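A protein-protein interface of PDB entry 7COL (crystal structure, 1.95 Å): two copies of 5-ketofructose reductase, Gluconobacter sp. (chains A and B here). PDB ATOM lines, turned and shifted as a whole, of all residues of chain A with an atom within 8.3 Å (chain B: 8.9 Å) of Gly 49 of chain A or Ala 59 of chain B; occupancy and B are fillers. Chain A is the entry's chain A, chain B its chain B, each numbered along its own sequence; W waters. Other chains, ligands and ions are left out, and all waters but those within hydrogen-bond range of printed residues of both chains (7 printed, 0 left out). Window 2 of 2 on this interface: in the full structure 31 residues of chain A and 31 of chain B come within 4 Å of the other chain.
Asp 52 of chain A touches Gly 56 of chain B, and with the chains exchanged Gly 56 of chain A touches Asp 52 of chain B.
Ala 53 of chain A touches Met 60 of chain B, and with the chains exchanged Met 60 of chain A touches Ala 53 of chain B.
Ala 57 of chain A touches Met 60 of chain B, and with the chains exchanged Met 60 of chain A touches Ala 57 of chain B.
Met 60 of chain B touches its own counterpart, Met 60 of chain A.
Positions printed for both chains: 52, 53, 54, 55, 56, 57 and 60.
Of the 24 pairs that touch across the chains among the printed residues, 12 have their exchanged pair printed and touching as well.
Ala 47 of chain A touches none of the printed residues of chain B.
Gly 49 of chain A touches just one residue of chain B: Ala 59.
Printed residues of chain B within 4 Å of Asp 52 of chain A: Lys 55, Gly 56 and Ala 59.
Of the printed residues of chain A, Lys 55 of chain B touches Asp 52 (3.8 Å).
Of chain A, only Asp 44, Val 45, Gly 49, Asp 52 and Ala 53 come within 4 Å of Ala 59 of chain B.
Leu 102 of chain B touches none of the printed residues of chain A.
The nearest residue of chain B that does not touch Gly 49 of chain A is Met 60 of chain B (5.8 Å).
The nearest residue of chain A that does not touch Ala 59 of chain B is Lys 46 of chain A (4.8 Å).
Water W1 bridges the side-chain carboxylate (OD1) of Asp 52 of chain A (2.6 Å) and the side-chain amino group (NZ) of Lys 55 of chain B (2.9 Å).
Water W4 lies within hydrogen-bond range of the side-chain amino group (NZ) of Lys 55 of chain A (2.6 Å), the side-chain carboxylate (OD1) of Asp 52 of chain A (2.9 Å), the side-chain carboxylate (OD1) of Asp 52 of chain B (3.1 Å) and the side-chain amino group (NZ) of Lys 55 of chain B (3.3 Å).
Water W5 lies within hydrogen-bond range of the backbone carbonyl oxygen (O) of Met 60 of chain B, the backbone NH (N) of Asp 44 of chain A and the guanidinium group (NH2) of Arg 7 of chain B.
Water W2 lies within hydrogen-bond range of O of Asp 52 of chain A (2.7 Å), O of Asp 52 of chain B (2.8 Å) and N of Gly 56 of chain A (3.0 Å).
Water W3 bridges O of Lys 55 of chain B (2.8 Å) and OD2 of Asp 52 of chain A (2.9 Å).
Water W6 lies within hydrogen-bond range of O of Lys 55 of chain A and OD2 of Asp 52 of chain B.
The side-chain amino group (NZ) of Lys 46 of chain A is in salt-bridge range of the side-chain carboxylate (OD1) of Asp 44 of chain A (2.7 Å).
The side-chain carboxylate of Glu 61 of chain B is in salt-bridge range of the guanidinium group of Arg 7 of chain B (2.6 Å).
The backbone carbonyl oxygen (O) of Cys 43 of chain A is in hydrogen-bond range of the backbone NH (N) of Ser 15 of chain A (3.4 Å).
O of Ala 57 of chain B sits at hydrogen-bond distance from N of Trp 62 of chain B (2.9 Å).
The side-chain amino group of Lys 55 of chain A is in salt-bridge range of the side-chain carboxylate of Asp 52 of chain A (3.6 Å).
The backbone carbonyl oxygen of Val 45 of chain A is in hydrogen-bond range of a ring nitrogen (NE2) of His 71 of chain A (2.7 Å).
CE1 of Phe 14 of chain A touches CG of Met 60 of chain B (3.9 Å).
Leu 10 of chain B touches Cys 43 of chain A.
SG of Cys 43 of chain A touches CG of Met 60 of chain B, 3.7 Å away.
Val 45 of chain A touches Ala 59 of chain B (CG2 to O, 3.7 Å).
Asp 52 of chain A touches Gly 56 of chain B.
CB of Ala 59 of chain B touches N of Ala 53 of chain A, 3.5 Å away.
Ala 53 of chain A touches Met 60 of chain B.
CE of Met 60 of chain B touches C of Gly 56 of chain A, at 3.8 Å.
Met 60 of chain B touches Met 60 of chain A (CE to CE, 3.7 Å).
Trp 62 of chain B touches Met 60 of chain A (CZ2 to SD, 3.8 Å).
NZ of Lys 46 of chain A lies within salt-bridge range of OE2 of Glu 61 of chain B, 2.6 Å away.
The side-chain carboxylate (OD2) of Asp 44 of chain A lies within salt-bridge range of the guanidinium group (NH1) of Arg 7 of chain B.
O of Asp 44 of chain A sits close to OE2 of Glu 61 of chain B (3.3 Å).
Of the 21 printed residues of chain A, 12 touch a printed residue of chain B.
Printed residues of chain A that touch a printed residue of chain B: Phe 14, Cys 43, Asp 44, Val 45, Lys 46, Gly 49, Asp 52, Ala 53, Lys 55, Gly 56, Ala 57 and Met 60.
Hydrophobic or aromatic side chains of chain A that line the printed part of chain B: Phe 14, Val 45, Ala 53 and Met 60.
Hydrophobic or aromatic side chains of chain B that line the printed part of chain A: Leu 10, Ala 59, Met 60 and Trp 62.
Among the printed residues, Asp or Glu carboxylates within 4 Å of a Lys or Arg side-chain nitrogen of the other chain: Asp 44 of chain A with Arg 7 of chain B (3.9 Å) and Lys 46 of chain A with Glu 61 of chain B (2.6 Å).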
ATOM      1  N   SER A  13     -16.988   5.418 -10.173  1.00  0.00           N
ATOM      2  CA  SER A  13     -18.172   4.622 -10.407  1.00  0.00           C
ATOM      3  C   SER A  13     -18.230   3.451  -9.439  1.00  0.00           C
ATOM      4  O   SER A  13     -17.216   2.781  -9.207  1.00  0.00           O
ATOM      5  CB  SER A  13     -18.137   4.064 -11.825  1.00  0.00           C
ATOM      6  OG  SER A  13     -19.388   3.470 -12.140  1.00  0.00           O
ATOM      7  N   PHE A  14     -19.420   3.214  -8.886  1.00  0.00           N
ATOM      8  CA  PHE A  14     -19.732   1.981  -8.168  1.00  0.00           C
ATOM      9  C   PHE A  14     -20.774   1.192  -8.943  1.00  0.00           C
ATOM     10  O   PHE A  14     -21.871   1.708  -9.225  1.00  0.00           O
ATOM     11  CB  PHE A  14     -20.256   2.274  -6.749  1.00  0.00           C
ATOM     12  CG  PHE A  14     -19.345   3.139  -5.920  1.00  0.00           C
ATOM     13  CD1 PHE A  14     -17.950   2.983  -5.967  1.00  0.00           C
ATOM     14  CD2 PHE A  14     -19.881   4.110  -5.077  1.00  0.00           C
ATOM     15  CE1 PHE A  14     -17.117   3.782  -5.188  1.00  0.00           C
ATOM     16  CE2 PHE A  14     -19.055   4.905  -4.287  1.00  0.00           C
ATOM     17  CZ  PHE A  14     -17.674   4.746  -4.346  1.00  0.00           C
ATOM     18  N   SER A  15     -20.429  -0.057  -9.280  1.00  0.00           N
ATOM     19  CA  SER A  15     -21.335  -0.962 -10.005  1.00  0.00           C
ATOM     20  C   SER A  15     -20.782  -2.389 -10.031  1.00  0.00           C
ATOM     21  O   SER A  15     -19.606  -2.625  -9.743  1.00  0.00           O
ATOM     22  CB  SER A  15     -21.557  -0.463 -11.440  1.00  0.00           C
ATOM     23  OG  SER A  15     -20.424  -0.734 -12.239  1.00  0.00           O
ATOM     24  N   CYS A  43     -15.003   1.230 -10.204  1.00  0.00           N
ATOM     25  CA  CYS A  43     -14.911   0.231  -9.128  1.00  0.00           C
ATOM     26  C   CYS A  43     -15.956  -0.847  -9.261  1.00  0.00           C
ATOM     27  O   CYS A  43     -17.112  -0.550  -9.518  1.00  0.00           O
ATOM     28  CB  CYS A  43     -15.083   0.886  -7.753  1.00  0.00           C
ATOM     29  SG  CYS A  43     -13.926   2.211  -7.389  1.00  0.00           S
ATOM     30  N   ASP A  44     -15.560  -2.099  -9.053  1.00  0.00           N
ATOM     31  CA  ASP A  44     -16.543  -3.168  -8.942  1.00  0.00           C
ATOM     32  C   ASP A  44     -16.935  -3.340  -7.470  1.00  0.00           C
ATOM     33  O   ASP A  44     -16.128  -3.763  -6.635  1.00  0.00           O
ATOM     34  CB  ASP A  44     -15.985  -4.464  -9.514  1.00  0.00           C
ATOM     35  CG  ASP A  44     -17.062  -5.447  -9.890  1.00  0.00           C
ATOM     36  OD1 ASP A  44     -17.798  -5.922  -9.005  1.00  0.00           O
ATOM     37  OD2 ASP A  44     -17.139  -5.774 -11.076  1.00  0.00           O
ATOM     38  N   VAL A  45     -18.176  -2.986  -7.164  1.00  0.00           N
ATOM     39  CA  VAL A  45     -18.647  -2.889  -5.787  1.00  0.00           C
ATOM     40  C   VAL A  45     -19.867  -3.782  -5.662  1.00  0.00           C
ATOM     41  O   VAL A  45     -20.900  -3.522  -6.298  1.00  0.00           O
ATOM     42  CB  VAL A  45     -19.008  -1.419  -5.400  1.00  0.00           C
ATOM     43  CG1 VAL A  45     -19.537  -1.341  -3.972  1.00  0.00           C
ATOM     44  CG2 VAL A  45     -17.821  -0.497  -5.557  1.00  0.00           C
ATOM     45  N   LYS A  46     -19.747  -4.836  -4.862  1.00  0.00           N
ATOM     46  CA  LYS A  46     -20.889  -5.722  -4.584  1.00  0.00           C
ATOM     47  C   LYS A  46     -21.888  -4.987  -3.694  1.00  0.00           C
ATOM     48  O   LYS A  46     -21.516  -4.007  -3.048  1.00  0.00           O
ATOM     49  CB  LYS A  46     -20.433  -7.045  -3.926  1.00  0.00           C
ATOM     50  CG  LYS A  46     -19.340  -7.824  -4.664  1.00  0.00           C
ATOM     51  CD  LYS A  46     -19.592  -7.980  -6.165  1.00  0.00           C
ATOM     52  CE  LYS A  46     -18.377  -8.527  -6.902  1.00  0.00           C
ATOM     53  NZ  LYS A  46     -17.231  -7.574  -6.924  1.00  0.00           N
ATOM     54  N   ALA A  47     -23.145  -5.438  -3.681  1.00  0.00           N
ATOM     55  CA  ALA A  47     -24.189  -4.876  -2.796  1.00  0.00           C
ATOM     56  C   ALA A  47     -23.810  -4.838  -1.307  1.00  0.00           C
ATOM     57  O   ALA A  47     -24.119  -3.875  -0.616  1.00  0.00           O
ATOM     58  CB  ALA A  47     -25.510  -5.602  -2.986  1.00  0.00           C
ATOM     59  N   SER A  48     -23.151  -5.886  -0.817  1.00  0.00           N
ATOM     60  CA  SER A  48     -22.582  -5.877   0.537  1.00  0.00           C
ATOM     61  C   SER A  48     -21.595  -4.724   0.797  1.00  0.00           C
ATOM     62  O   SER A  48     -21.437  -4.294   1.948  1.00  0.00           O
ATOM     63  CB  SER A  48     -21.921  -7.214   0.854  1.00  0.00           C
ATOM     64  OG  SER A  48     -20.673  -7.316   0.203  1.00  0.00           O
ATOM     65  N   GLY A  49     -20.963  -4.213  -0.264  1.00  0.00           N
ATOM     66  CA  GLY A  49     -19.971  -3.137  -0.136  1.00  0.00           C
ATOM     67  C   GLY A  49     -20.419  -1.715  -0.439  1.00  0.00           C
ATOM     68  O   GLY A  49     -19.642  -0.780  -0.271  1.00  0.00           O
ATOM     69  N   LEU A  50     -21.667  -1.544  -0.883  1.00  0.00           N
ATOM     70  CA  LEU A  50     -22.169  -0.233  -1.269  1.00  0.00           C
ATOM     71  C   LEU A  50     -22.061   0.824  -0.177  1.00  0.00           C
ATOM     72  O   LEU A  50     -21.570   1.919  -0.449  1.00  0.00           O
ATOM     73  CB  LEU A  50     -23.608  -0.312  -1.807  1.00  0.00           C
ATOM     74  CG  LEU A  50     -24.140   0.994  -2.401  1.00  0.00           C
ATOM     75  CD1 LEU A  50     -23.311   1.439  -3.613  1.00  0.00           C
ATOM     76  CD2 LEU A  50     -25.613   0.837  -2.751  1.00  0.00           C
ATOM     77  N   ALA A  51     -22.505   0.501   1.044  1.00  0.00           N
ATOM     78  CA  ALA A  51     -22.443   1.451   2.150  1.00  0.00           C
ATOM     79  C   ALA A  51     -21.001   1.923   2.380  1.00  0.00           C
ATOM     80  O   ALA A  51     -20.736   3.140   2.359  1.00  0.00           O
ATOM     81  CB  ALA A  51     -23.052   0.870   3.430  1.00  0.00           C
ATOM     82  N   ASP A  52     -20.068   0.977   2.523  1.00  0.00           N
ATOM     83  CA  ASP A  52     -18.645   1.350   2.766  1.00  0.00           C
ATOM     84  C   ASP A  52     -17.981   2.032   1.565  1.00  0.00           C
ATOM     85  O   ASP A  52     -17.028   2.790   1.739  1.00  0.00           O
ATOM     86  CB  ASP A  52     -17.811   0.147   3.171  1.00  0.00           C
ATOM     87  CG  ASP A  52     -18.189  -0.403   4.528  1.00  0.00           C
ATOM     88  OD1 ASP A  52     -18.904   0.272   5.284  1.00  0.00           O
ATOM     89  OD2 ASP A  52     -17.754  -1.526   4.830  1.00  0.00           O
ATOM     90  N   ALA A  53     -18.457   1.741   0.357  1.00  0.00           N
ATOM     91  CA  ALA A  53     -17.918   2.390  -0.831  1.00  0.00           C
ATOM     92  C   ALA A  53     -18.291   3.867  -0.831  1.00  0.00           C
ATOM     93  O   ALA A  53     -17.439   4.712  -1.067  1.00  0.00           O
ATOM     94  CB  ALA A  53     -18.389   1.687  -2.106  1.00  0.00           C
ATOM     95  N   VAL A  54     -19.561   4.166  -0.537  1.00  0.00           N
ATOM     96  CA  VAL A  54     -20.065   5.545  -0.452  1.00  0.00           C
ATOM     97  C   VAL A  54     -19.330   6.345   0.642  1.00  0.00           C
ATOM     98  O   VAL A  54     -18.847   7.457   0.400  1.00  0.00           O
ATOM     99  CB  VAL A  54     -21.618   5.568  -0.297  1.00  0.00           C
ATOM    100  CG1 VAL A  54     -22.141   6.980  -0.089  1.00  0.00           C
ATOM    101  CG2 VAL A  54     -22.287   4.959  -1.524  1.00  0.00           C
ATOM    102  N   LYS A  55     -19.227   5.767   1.831  1.00  0.00           N
ATOM    103  CA  LYS A  55     -18.493   6.397   2.932  1.00  0.00           C
ATOM    104  C   LYS A  55     -16.997   6.437   2.674  1.00  0.00           C
ATOM    105  O   LYS A  55     -16.320   7.340   3.146  1.00  0.00           O
ATOM    106  CB  LYS A  55     -18.814   5.720   4.274  1.00  0.00           C
ATOM    107  CG  LYS A  55     -20.167   6.150   4.815  1.00  0.00           C
ATOM    108  CD  LYS A  55     -20.344   5.919   6.310  1.00  0.00           C
ATOM    109  CE  LYS A  55     -21.091   4.626   6.579  1.00  0.00           C
ATOM    110  NZ  LYS A  55     -20.184   3.448   6.431  1.00  0.00           N
ATOM    111  N   GLY A  56     -16.513   5.457   1.907  1.00  0.00           N
ATOM    112  CA  GLY A  56     -15.155   5.430   1.365  1.00  0.00           C
ATOM    113  C   GLY A  56     -14.840   6.605   0.454  1.00  0.00           C
ATOM    114  O   GLY A  56     -13.797   7.236   0.621  1.00  0.00           O
ATOM    115  N   ALA A  57     -15.737   6.909  -0.493  1.00  0.00           N
ATOM    116  CA  ALA A  57     -15.537   8.076  -1.386  1.00  0.00           C
ATOM    117  C   ALA A  57     -15.506   9.401  -0.599  1.00  0.00           C
ATOM    118  O   ALA A  57     -14.775  10.315  -0.937  1.00  0.00           O
ATOM    119  CB  ALA A  57     -16.608   8.116  -2.479  1.00  0.00           C
ATOM    120  N   MET A  60     -12.130   9.522   1.319  1.00  0.00           N
ATOM    121  CA  MET A  60     -11.049   9.673   0.357  1.00  0.00           C
ATOM    122  C   MET A  60     -11.149  11.011  -0.353  1.00  0.00           C
ATOM    123  O   MET A  60     -10.353  11.309  -1.264  1.00  0.00           O
ATOM    124  CB  MET A  60     -11.072   8.539  -0.675  1.00  0.00           C
ATOM    125  CG  MET A  60     -10.615   7.169  -0.179  1.00  0.00           C
ATOM    126  SD  MET A  60     -10.998   5.975  -1.467  1.00  0.00           S
ATOM    127  CE  MET A  60     -11.073   4.430  -0.558  1.00  0.00           C
ATOM    128  N   HIS A  71     -26.985  -0.631  -7.997  1.00  0.00           N
ATOM    129  CA  HIS A  71     -26.941   0.300  -6.859  1.00  0.00           C
ATOM    130  C   HIS A  71     -27.881   1.521  -6.915  1.00  0.00           C
ATOM    131  O   HIS A  71     -27.974   2.275  -5.929  1.00  0.00           O
ATOM    132  CB  HIS A  71     -25.502   0.790  -6.633  1.00  0.00           C
ATOM    133  CG  HIS A  71     -24.509  -0.306  -6.409  1.00  0.00           C
ATOM    134  ND1 HIS A  71     -24.750  -1.376  -5.569  1.00  0.00           N
ATOM    135  CD2 HIS A  71     -23.255  -0.478  -6.888  1.00  0.00           C
ATOM    136  CE1 HIS A  71     -23.691  -2.164  -5.553  1.00  0.00           C
ATOM    137  NE2 HIS A  71     -22.771  -1.646  -6.348  1.00  0.00           N
ATOM    138  N   HIS A  78     -28.078   5.970   1.629  1.00  0.00           N
ATOM    139  CA  HIS A  78     -26.775   6.493   2.046  1.00  0.00           C
ATOM    140  C   HIS A  78     -26.615   7.982   1.730  1.00  0.00           C
ATOM    141  O   HIS A  78     -25.542   8.549   1.962  1.00  0.00           O
ATOM    142  CB  HIS A  78     -25.621   5.660   1.446  1.00  0.00           C
ATOM    143  CG  HIS A  78     -25.789   4.180   1.608  1.00  0.00           C
ATOM    144  ND1 HIS A  78     -25.915   3.570   2.839  1.00  0.00           N
ATOM    145  CD2 HIS A  78     -25.857   3.187   0.689  1.00  0.00           C
ATOM    146  CE1 HIS A  78     -26.074   2.270   2.670  1.00  0.00           C
ATOM    147  NE2 HIS A  78     -26.028   2.009   1.375  1.00  0.00           N
ATOM    148  N   ARG B   7     -12.153  -2.370 -16.159  1.00  0.00           N
ATOM    149  CA  ARG B   7     -11.793  -2.459 -14.758  1.00  0.00           C
ATOM    150  C   ARG B   7     -10.262  -2.518 -14.651  1.00  0.00           C
ATOM    151  O   ARG B   7      -9.618  -3.356 -15.274  1.00  0.00           O
ATOM    152  CB  ARG B   7     -12.440  -3.694 -14.118  1.00  0.00           C
ATOM    153  CG  ARG B   7     -12.180  -3.796 -12.625  1.00  0.00           C
ATOM    154  CD  ARG B   7     -12.548  -5.152 -12.059  1.00  0.00           C
ATOM    155  NE  ARG B   7     -12.481  -5.109 -10.601  1.00  0.00           N
ATOM    156  CZ  ARG B   7     -12.978  -6.027  -9.764  1.00  0.00           C
ATOM    157  NH1 ARG B   7     -13.611  -7.115 -10.207  1.00  0.00           N
ATOM    158  NH2 ARG B   7     -12.855  -5.841  -8.459  1.00  0.00           N
ATOM    159  N   LEU B  10      -6.833  -1.880  -8.675  1.00  0.00           N
ATOM    160  CA  LEU B  10      -6.760  -0.656  -7.888  1.00  0.00           C
ATOM    161  C   LEU B  10      -5.822  -0.716  -6.706  1.00  0.00           C
ATOM    162  O   LEU B  10      -5.914  -1.610  -5.835  1.00  0.00           O
ATOM    163  CB  LEU B  10      -8.151  -0.195  -7.450  1.00  0.00           C
ATOM    164  CG  LEU B  10      -9.129   0.110  -8.587  1.00  0.00           C
ATOM    165  CD1 LEU B  10     -10.505   0.401  -8.006  1.00  0.00           C
ATOM    166  CD2 LEU B  10      -8.639   1.271  -9.468  1.00  0.00           C
ATOM    167  N   ASP B  52     -12.968   4.871   7.685  1.00  0.00           N
ATOM    168  CA  ASP B  52     -13.851   4.799   6.521  1.00  0.00           C
ATOM    169  C   ASP B  52     -13.074   4.677   5.206  1.00  0.00           C
ATOM    170  O   ASP B  52     -13.544   4.007   4.296  1.00  0.00           O
ATOM    171  CB  ASP B  52     -14.835   5.971   6.482  1.00  0.00           C
ATOM    172  CG  ASP B  52     -15.969   5.829   7.495  1.00  0.00           C
ATOM    173  OD1 ASP B  52     -16.125   4.761   8.138  1.00  0.00           O
ATOM    174  OD2 ASP B  52     -16.724   6.804   7.652  1.00  0.00           O
ATOM    175  N   ALA B  53     -11.878   5.268   5.117  1.00  0.00           N
ATOM    176  CA  ALA B  53     -11.076   5.138   3.871  1.00  0.00           C
ATOM    177  C   ALA B  53     -10.608   3.695   3.680  1.00  0.00           C
ATOM    178  O   ALA B  53     -10.701   3.136   2.578  1.00  0.00           O
ATOM    179  CB  ALA B  53      -9.907   6.107   3.833  1.00  0.00           C
ATOM    180  N   VAL B  54     -10.135   3.094   4.766  1.00  0.00           N
ATOM    181  CA  VAL B  54      -9.752   1.679   4.786  1.00  0.00           C
ATOM    182  C   VAL B  54     -10.910   0.772   4.327  1.00  0.00           C
ATOM    183  O   VAL B  54     -10.739  -0.043   3.409  1.00  0.00           O
ATOM    184  CB  VAL B  54      -9.179   1.310   6.177  1.00  0.00           C
ATOM    185  CG1 VAL B  54      -9.294  -0.174   6.484  1.00  0.00           C
ATOM    186  CG2 VAL B  54      -7.738   1.770   6.263  1.00  0.00           C
ATOM    187  N   LYS B  55     -12.078   0.952   4.937  1.00  0.00           N
ATOM    188  CA  LYS B  55     -13.290   0.221   4.550  1.00  0.00           C
ATOM    189  C   LYS B  55     -13.675   0.498   3.090  1.00  0.00           C
ATOM    190  O   LYS B  55     -14.092  -0.408   2.382  1.00  0.00           O
ATOM    191  CB  LYS B  55     -14.444   0.554   5.497  1.00  0.00           C
ATOM    192  CG  LYS B  55     -14.393  -0.168   6.831  1.00  0.00           C
ATOM    193  CD  LYS B  55     -15.086   0.678   7.886  1.00  0.00           C
ATOM    194  CE  LYS B  55     -16.068  -0.137   8.697  1.00  0.00           C
ATOM    195  NZ  LYS B  55     -17.139   0.758   9.217  1.00  0.00           N
ATOM    196  N   GLY B  56     -13.490   1.745   2.649  1.00  0.00           N
ATOM    197  CA  GLY B  56     -13.622   2.129   1.249  1.00  0.00           C
ATOM    198  C   GLY B  56     -12.804   1.286   0.302  1.00  0.00           C
ATOM    199  O   GLY B  56     -13.342   0.706  -0.640  1.00  0.00           O
ATOM    200  N   ALA B  57     -11.502   1.205   0.577  1.00  0.00           N
ATOM    201  CA  ALA B  57     -10.568   0.416  -0.215  1.00  0.00           C
ATOM    202  C   ALA B  57     -10.997  -1.048  -0.335  1.00  0.00           C
ATOM    203  O   ALA B  57     -10.936  -1.634  -1.426  1.00  0.00           O
ATOM    204  CB  ALA B  57      -9.158   0.528   0.371  1.00  0.00           C
ATOM    205  N   LYS B  58     -11.470  -1.618   0.773  1.00  0.00           N
ATOM    206  CA  LYS B  58     -11.988  -2.976   0.755  1.00  0.00           C
ATOM    207  C   LYS B  58     -13.272  -3.096  -0.077  1.00  0.00           C
ATOM    208  O   LYS B  58     -13.399  -4.021  -0.872  1.00  0.00           O
ATOM    209  CB  LYS B  58     -12.249  -3.443   2.171  1.00  0.00           C
ATOM    210  CG  LYS B  58     -12.503  -4.937   2.309  1.00  0.00           C
ATOM    211  CD  LYS B  58     -12.974  -5.256   3.719  1.00  0.00           C
ATOM    212  CE  LYS B  58     -11.845  -5.077   4.727  1.00  0.00           C
ATOM    213  NZ  LYS B  58     -12.426  -5.073   6.094  1.00  0.00           N
ATOM    214  N   ALA B  59     -14.206  -2.162   0.097  1.00  0.00           N
ATOM    215  CA  ALA B  59     -15.477  -2.175  -0.663  1.00  0.00           C
ATOM    216  C   ALA B  59     -15.271  -1.956  -2.182  1.00  0.00           C
ATOM    217  O   ALA B  59     -15.992  -2.532  -3.005  1.00  0.00           O
ATOM    218  CB  ALA B  59     -16.415  -1.122  -0.101  1.00  0.00           C
ATOM    219  N   MET B  60     -14.286  -1.126  -2.542  1.00  0.00           N
ATOM    220  CA  MET B  60     -13.956  -0.805  -3.944  1.00  0.00           C
ATOM    221  C   MET B  60     -13.021  -1.834  -4.567  1.00  0.00           C
ATOM    222  O   MET B  60     -12.567  -1.669  -5.708  1.00  0.00           O
ATOM    223  CB  MET B  60     -13.299   0.564  -4.022  1.00  0.00           C
ATOM    224  CG  MET B  60     -14.224   1.710  -3.702  1.00  0.00           C
ATOM    225  SD  MET B  60     -13.282   3.232  -3.653  1.00  0.00           S
ATOM    226  CE  MET B  60     -14.244   4.125  -2.423  1.00  0.00           C
ATOM    227  N   GLU B  61     -12.726  -2.868  -3.776  1.00  0.00           N
ATOM    228  CA  GLU B  61     -11.888  -4.010  -4.134  1.00  0.00           C
ATOM    229  C   GLU B  61     -10.465  -3.680  -4.562  1.00  0.00           C
ATOM    230  O   GLU B  61      -9.913  -4.272  -5.496  1.00  0.00           O
ATOM    231  CB  GLU B  61     -12.616  -4.925  -5.124  1.00  0.00           C
ATOM    232  CG  GLU B  61     -13.645  -5.799  -4.421  1.00  0.00           C
ATOM    233  CD  GLU B  61     -14.543  -6.547  -5.368  1.00  0.00           C
ATOM    234  OE1 GLU B  61     -14.084  -7.011  -6.438  1.00  0.00           O
ATOM    235  OE2 GLU B  61     -15.726  -6.656  -5.038  1.00  0.00           O
ATOM    236  N   TRP B  62      -9.872  -2.724  -3.856  1.00  0.00           N
ATOM    237  CA  TRP B  62      -8.442  -2.443  -3.990  1.00  0.00           C
ATOM    238  C   TRP B  62      -7.677  -3.662  -3.516  1.00  0.00           C
ATOM    239  O   TRP B  62      -8.187  -4.434  -2.707  1.00  0.00           O
ATOM    240  CB  TRP B  62      -8.041  -1.250  -3.130  1.00  0.00           C
ATOM    241  CG  TRP B  62      -8.612   0.085  -3.504  1.00  0.00           C
ATOM    242  CD1 TRP B  62      -9.801   0.343  -4.168  1.00  0.00           C
ATOM    243  CD2 TRP B  62      -8.066   1.357  -3.160  1.00  0.00           C
ATOM    244  NE1 TRP B  62      -9.986   1.698  -4.286  1.00  0.00           N
ATOM    245  CE2 TRP B  62      -8.950   2.341  -3.653  1.00  0.00           C
ATOM    246  CE3 TRP B  62      -6.902   1.767  -2.477  1.00  0.00           C
ATOM    247  CZ2 TRP B  62      -8.698   3.711  -3.509  1.00  0.00           C
ATOM    248  CZ3 TRP B  62      -6.668   3.128  -2.310  1.00  0.00           C
ATOM    249  CH2 TRP B  62      -7.557   4.085  -2.830  1.00  0.00           C
ATOM    250  N   ILE B  97      -4.516  -6.076   0.722  1.00  0.00           N
ATOM    251  CA  ILE B  97      -5.875  -6.607   0.858  1.00  0.00           C
ATOM    252  C   ILE B  97      -5.888  -8.000   0.198  1.00  0.00           C
ATOM    253  O   ILE B  97      -5.765  -8.125  -1.028  1.00  0.00           O
ATOM    254  CB  ILE B  97      -6.967  -5.652   0.292  1.00  0.00           C
ATOM    255  CG1 ILE B  97      -6.702  -4.199   0.741  1.00  0.00           C
ATOM    256  CG2 ILE B  97      -8.361  -6.142   0.693  1.00  0.00           C
ATOM    257  CD1 ILE B  97      -7.771  -3.175   0.367  1.00  0.00           C
ATOM    258  N   GLY B 100     -10.214 -10.057   1.223  1.00  0.00           N
ATOM    259  CA  GLY B 100     -10.948  -9.132   2.102  1.00  0.00           C
ATOM    260  C   GLY B 100     -10.324  -8.845   3.464  1.00  0.00           C
ATOM    261  O   GLY B 100     -10.952  -8.204   4.309  1.00  0.00           O
ATOM    262  N   LEU B 102      -6.932  -7.447   5.810  1.00  0.00           N
ATOM    263  CA  LEU B 102      -5.890  -6.425   5.750  1.00  0.00           C
ATOM    264  C   LEU B 102      -4.644  -6.855   6.503  1.00  0.00           C
ATOM    265  O   LEU B 102      -4.695  -7.195   7.694  1.00  0.00           O
ATOM    266  CB  LEU B 102      -6.390  -5.098   6.284  1.00  0.00           C
ATOM    267  CG  LEU B 102      -7.698  -4.483   5.779  1.00  0.00           C
ATOM    268  CD1 LEU B 102      -7.637  -3.042   6.214  1.00  0.00           C
ATOM    269  CD2 LEU B 102      -7.919  -4.554   4.274  1.00  0.00           C
HETATM  270  O   HOH W   1     -18.979  -0.778   7.623  1.00  0.00           O
HETATM  271  O   HOH W   2     -16.304   3.506   4.239  1.00  0.00           O
HETATM  272  O   HOH W   3     -15.429  -2.573   3.511  1.00  0.00           O
HETATM  273  O   HOH W   4     -17.706   2.600   6.574  1.00  0.00           O
HETATM  274  O   HOH W   5     -12.938  -2.588  -8.197  1.00  0.00           O
HETATM  275  O   HOH W   6     -17.059   8.793   5.494  1.00  0.00           O
HETATM  276  O   HOH W   7     -17.398  -4.912  -3.380  1.00  0.00           O
